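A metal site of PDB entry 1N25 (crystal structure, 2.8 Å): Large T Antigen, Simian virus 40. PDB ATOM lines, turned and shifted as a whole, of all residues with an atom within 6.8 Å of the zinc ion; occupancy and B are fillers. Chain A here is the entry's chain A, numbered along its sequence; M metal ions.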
ATOM      1  N   GLU A  35     -14.334 -15.209  29.854  1.00  0.00           N
ATOM      2  CA  GLU A  35     -13.083 -15.429  29.154  1.00  0.00           C
ATOM      3  C   GLU A  35     -12.984 -16.894  28.748  1.00  0.00           C
ATOM      4  O   GLU A  35     -12.363 -17.230  27.739  1.00  0.00           O
ATOM      5  CB  GLU A  35     -11.895 -15.060  30.017  1.00  0.00           C
ATOM      6  CG  GLU A  35     -11.872 -13.614  30.428  1.00  0.00           C
ATOM      7  CD  GLU A  35     -10.511 -13.159  30.893  1.00  0.00           C
ATOM      8  OE1 GLU A  35      -9.921 -13.840  31.768  1.00  0.00           O
ATOM      9  OE2 GLU A  35     -10.046 -12.118  30.386  1.00  0.00           O
ATOM     10  N   PHE A  36     -13.609 -17.759  29.558  1.00  0.00           N
ATOM     11  CA  PHE A  36     -13.608 -19.203  29.319  1.00  0.00           C
ATOM     12  C   PHE A  36     -14.431 -19.651  28.101  1.00  0.00           C
ATOM     13  O   PHE A  36     -14.285 -20.778  27.635  1.00  0.00           O
ATOM     14  CB  PHE A  36     -14.156 -19.948  30.553  1.00  0.00           C
ATOM     15  CG  PHE A  36     -13.461 -19.613  31.854  1.00  0.00           C
ATOM     16  CD1 PHE A  36     -12.124 -19.243  31.885  1.00  0.00           C
ATOM     17  CD2 PHE A  36     -14.131 -19.748  33.061  1.00  0.00           C
ATOM     18  CE1 PHE A  36     -11.470 -19.017  33.107  1.00  0.00           C
ATOM     19  CE2 PHE A  36     -13.490 -19.516  34.284  1.00  0.00           C
ATOM     20  CZ  PHE A  36     -12.161 -19.161  34.304  1.00  0.00           C
ATOM     21  N   TYR A  38     -14.080 -19.270  25.142  1.00  0.00           N
ATOM     22  CA  TYR A  38     -13.295 -19.562  23.959  1.00  0.00           C
ATOM     23  C   TYR A  38     -12.643 -20.919  24.115  1.00  0.00           C
ATOM     24  O   TYR A  38     -12.380 -21.362  25.236  1.00  0.00           O
ATOM     25  CB  TYR A  38     -12.223 -18.500  23.783  1.00  0.00           C
ATOM     26  CG  TYR A  38     -12.794 -17.107  23.730  1.00  0.00           C
ATOM     27  CD1 TYR A  38     -13.593 -16.704  22.661  1.00  0.00           C
ATOM     28  CD2 TYR A  38     -12.531 -16.198  24.748  1.00  0.00           C
ATOM     29  CE1 TYR A  38     -14.105 -15.425  22.605  1.00  0.00           C
ATOM     30  CE2 TYR A  38     -13.047 -14.911  24.702  1.00  0.00           C
ATOM     31  CZ  TYR A  38     -13.831 -14.528  23.634  1.00  0.00           C
ATOM     32  OH  TYR A  38     -14.317 -13.245  23.593  1.00  0.00           O
ATOM     33  N   SER A  39     -12.393 -21.600  23.007  1.00  0.00           N
ATOM     34  CA  SER A  39     -11.783 -22.923  23.083  1.00  0.00           C
ATOM     35  C   SER A  39     -10.458 -22.763  23.802  1.00  0.00           C
ATOM     36  O   SER A  39      -9.633 -21.905  23.443  1.00  0.00           O
ATOM     37  CB  SER A  39     -11.547 -23.516  21.700  1.00  0.00           C
ATOM     38  OG  SER A  39     -10.294 -23.122  21.174  1.00  0.00           O
ATOM     39  N   PHE A  40     -10.280 -23.585  24.837  1.00  0.00           N
ATOM     40  CA  PHE A  40      -9.056 -23.564  25.622  1.00  0.00           C
ATOM     41  C   PHE A  40      -8.004 -24.279  24.778  1.00  0.00           C
ATOM     42  O   PHE A  40      -6.802 -24.141  24.996  1.00  0.00           O
ATOM     43  CB  PHE A  40      -9.304 -24.295  26.940  1.00  0.00           C
ATOM     44  CG  PHE A  40      -8.534 -25.573  27.091  1.00  0.00           C
ATOM     45  CD1 PHE A  40      -7.372 -25.604  27.841  1.00  0.00           C
ATOM     46  CD2 PHE A  40      -8.971 -26.739  26.478  1.00  0.00           C
ATOM     47  CE1 PHE A  40      -6.637 -26.780  27.977  1.00  0.00           C
ATOM     48  CE2 PHE A  40      -8.248 -27.924  26.598  1.00  0.00           C
ATOM     49  CZ  PHE A  40      -7.083 -27.948  27.354  1.00  0.00           C
ATOM     50  N   CYS A  43      -6.233 -21.262  23.857  1.00  0.00           N
ATOM     51  CA  CYS A  43      -6.098 -20.158  24.821  1.00  0.00           C
ATOM     52  C   CYS A  43      -4.634 -19.845  25.160  1.00  0.00           C
ATOM     53  O   CYS A  43      -3.953 -20.651  25.797  1.00  0.00           O
ATOM     54  CB  CYS A  43      -6.871 -20.473  26.119  1.00  0.00           C
ATOM     55  SG  CYS A  43      -6.409 -19.561  27.634  1.00  0.00           S
ATOM     56  N   LEU A  44      -4.160 -18.679  24.710  1.00  0.00           N
ATOM     57  CA  LEU A  44      -2.786 -18.266  24.997  1.00  0.00           C
ATOM     58  C   LEU A  44      -2.640 -17.848  26.445  1.00  0.00           C
ATOM     59  O   LEU A  44      -1.556 -17.975  27.025  1.00  0.00           O
ATOM     60  CB  LEU A  44      -2.364 -17.103  24.087  1.00  0.00           C
ATOM     61  CG  LEU A  44      -1.656 -17.474  22.785  1.00  0.00           C
ATOM     62  CD1 LEU A  44      -1.161 -16.216  22.087  1.00  0.00           C
ATOM     63  CD2 LEU A  44      -0.460 -18.390  23.089  1.00  0.00           C
ATOM     64  N   LYS A  45      -3.734 -17.369  27.036  1.00  0.00           N
ATOM     65  CA  LYS A  45      -3.753 -16.939  28.442  1.00  0.00           C
ATOM     66  C   LYS A  45      -3.412 -18.123  29.316  1.00  0.00           C
ATOM     67  O   LYS A  45      -2.820 -17.975  30.389  1.00  0.00           O
ATOM     68  CB  LYS A  45      -5.130 -16.400  28.805  1.00  0.00           C
ATOM     69  CG  LYS A  45      -5.541 -15.186  27.992  1.00  0.00           C
ATOM     70  CD  LYS A  45      -6.735 -14.450  28.571  1.00  0.00           C
ATOM     71  CE  LYS A  45      -6.996 -13.189  27.758  1.00  0.00           C
ATOM     72  NZ  LYS A  45      -8.196 -12.437  28.204  1.00  0.00           N
ATOM     73  N   CYS A  46      -3.792 -19.298  28.851  1.00  0.00           N
ATOM     74  CA  CYS A  46      -3.544 -20.559  29.537  1.00  0.00           C
ATOM     75  C   CYS A  46      -2.153 -21.067  29.195  1.00  0.00           C
ATOM     76  O   CYS A  46      -1.370 -21.379  30.081  1.00  0.00           O
ATOM     77  CB  CYS A  46      -4.569 -21.590  29.078  1.00  0.00           C
ATOM     78  SG  CYS A  46      -6.282 -20.993  29.118  1.00  0.00           S
ATOM     79  N   ILE A  47      -1.863 -21.136  27.894  1.00  0.00           N
ATOM     80  CA  ILE A  47      -0.554 -21.589  27.427  1.00  0.00           C
ATOM     81  C   ILE A  47       0.525 -20.764  28.101  1.00  0.00           C
ATOM     82  O   ILE A  47       1.514 -21.298  28.626  1.00  0.00           O
ATOM     83  CB  ILE A  47      -0.395 -21.449  25.881  1.00  0.00           C
ATOM     84  CG1 ILE A  47      -1.433 -22.299  25.159  1.00  0.00           C
ATOM     85  CG2 ILE A  47       1.009 -21.901  25.466  1.00  0.00           C
ATOM     86  CD1 ILE A  47      -1.370 -22.192  23.650  1.00  0.00           C
ATOM     87  N   HIS A  54      -7.433 -17.905  35.908  1.00  0.00           N
ATOM     88  CA  HIS A  54      -7.905 -18.254  34.593  1.00  0.00           C
ATOM     89  C   HIS A  54      -7.356 -19.607  34.101  1.00  0.00           C
ATOM     90  O   HIS A  54      -8.123 -20.533  33.811  1.00  0.00           O
ATOM     91  CB  HIS A  54      -7.503 -17.169  33.602  1.00  0.00           C
ATOM     92  CG  HIS A  54      -7.858 -17.485  32.180  1.00  0.00           C
ATOM     93  ND1 HIS A  54      -9.147 -17.381  31.695  1.00  0.00           N
ATOM     94  CD2 HIS A  54      -7.102 -17.918  31.150  1.00  0.00           C
ATOM     95  CE1 HIS A  54      -9.161 -17.739  30.415  1.00  0.00           C
ATOM     96  NE2 HIS A  54      -7.926 -18.068  30.063  1.00  0.00           N
ATOM     97  N   TYR A  55      -6.036 -19.707  34.022  1.00  0.00           N
ATOM     98  CA  TYR A  55      -5.423 -20.924  33.514  1.00  0.00           C
ATOM     99  C   TYR A  55      -5.581 -22.212  34.320  1.00  0.00           C
ATOM    100  O   TYR A  55      -5.008 -23.228  33.961  1.00  0.00           O
ATOM    101  CB  TYR A  55      -3.935 -20.653  33.227  1.00  0.00           C
ATOM    102  CG  TYR A  55      -3.047 -20.581  34.447  1.00  0.00           C
ATOM    103  CD1 TYR A  55      -2.863 -21.681  35.281  1.00  0.00           C
ATOM    104  CD2 TYR A  55      -2.332 -19.412  34.734  1.00  0.00           C
ATOM    105  CE1 TYR A  55      -1.993 -21.638  36.364  1.00  0.00           C
ATOM    106  CE2 TYR A  55      -1.458 -19.362  35.823  1.00  0.00           C
ATOM    107  CZ  TYR A  55      -1.296 -20.473  36.630  1.00  0.00           C
ATOM    108  OH  TYR A  55      -0.435 -20.433  37.685  1.00  0.00           O
ATOM    109  N   TYR A  57      -8.843 -23.014  35.399  1.00  0.00           N
ATOM    110  CA  TYR A  57     -10.254 -23.333  35.283  1.00  0.00           C
ATOM    111  C   TYR A  57     -10.807 -23.261  33.873  1.00  0.00           C
ATOM    112  O   TYR A  57     -11.922 -23.739  33.625  1.00  0.00           O
ATOM    113  CB  TYR A  57     -11.067 -22.398  36.194  1.00  0.00           C
ATOM    114  CG  TYR A  57     -10.608 -22.368  37.629  1.00  0.00           C
ATOM    115  CD1 TYR A  57      -9.507 -21.608  38.021  1.00  0.00           C
ATOM    116  CD2 TYR A  57     -11.258 -23.129  38.610  1.00  0.00           C
ATOM    117  CE1 TYR A  57      -9.060 -21.597  39.359  1.00  0.00           C
ATOM    118  CE2 TYR A  57     -10.824 -23.128  39.931  1.00  0.00           C
ATOM    119  CZ  TYR A  57      -9.729 -22.363  40.301  1.00  0.00           C
ATOM    120  OH  TYR A  57      -9.289 -22.382  41.612  1.00  0.00           O
ATOM    121  N   HIS A  58     -10.055 -22.684  32.947  1.00  0.00           N
ATOM    122  CA  HIS A  58     -10.541 -22.565  31.576  1.00  0.00           C
ATOM    123  C   HIS A  58     -10.984 -23.916  31.014  1.00  0.00           C
ATOM    124  O   HIS A  58     -12.084 -24.032  30.463  1.00  0.00           O
ATOM    125  CB  HIS A  58      -9.480 -21.948  30.651  1.00  0.00           C
ATOM    126  CG  HIS A  58     -10.019 -21.572  29.295  1.00  0.00           C
ATOM    127  ND1 HIS A  58      -9.243 -20.986  28.321  1.00  0.00           N
ATOM    128  CD2 HIS A  58     -11.268 -21.678  28.772  1.00  0.00           C
ATOM    129  CE1 HIS A  58      -9.984 -20.740  27.256  1.00  0.00           C
ATOM    130  NE2 HIS A  58     -11.218 -21.149  27.504  1.00  0.00           N
ATOM    131  N   GLU A  59     -10.130 -24.919  31.157  1.00  0.00           N
ATOM    132  CA  GLU A  59     -10.420 -26.260  30.671  1.00  0.00           C
ATOM    133  C   GLU A  59     -11.783 -26.713  31.185  1.00  0.00           C
ATOM    134  O   GLU A  59     -12.748 -26.833  30.435  1.00  0.00           O
ATOM    135  CB  GLU A  59      -9.339 -27.233  31.176  1.00  0.00           C
ATOM    136  CG  GLU A  59      -8.719 -28.135  30.113  1.00  0.00           C
ATOM    137  CD  GLU A  59      -9.723 -29.077  29.468  1.00  0.00           C
ATOM    138  OE1 GLU A  59      -9.283 -29.963  28.695  1.00  0.00           O
ATOM    139  OE2 GLU A  59     -10.936 -28.941  29.730  1.00  0.00           O
HETATM  140 ZN    ZN M   1      -7.863 -19.926  29.058  1.00  0.00          ZN
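O of Phe 36 is in hydrogen-bond range of NE2 of His 58 (3.1 Å).
O of Tyr 38 sits at hydrogen-bond distance from NE2 of His 58.
The side-chain sulfur (SG) of Cys 43 is disulfide-bonded to the side-chain sulfur (SG) of Cys 46, 2.1 Å away.
N of Lys 45 sits close to SG of Cys 43.
Of the 15 residues printed, 4 come within 4 Å of the zinc ion.
ND1 of His 58 is bound to the zinc ion, at 1.9 Å.
The zinc ion is bound by SG of Cys 46 (1.9 Å).
SG of Cys 43 is bound to the zinc ion (2.1 Å).
NE2 of His 54 is bound to the zinc ion, 2.1 Å away.
The zinc ion has four donor atoms within binding distance.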
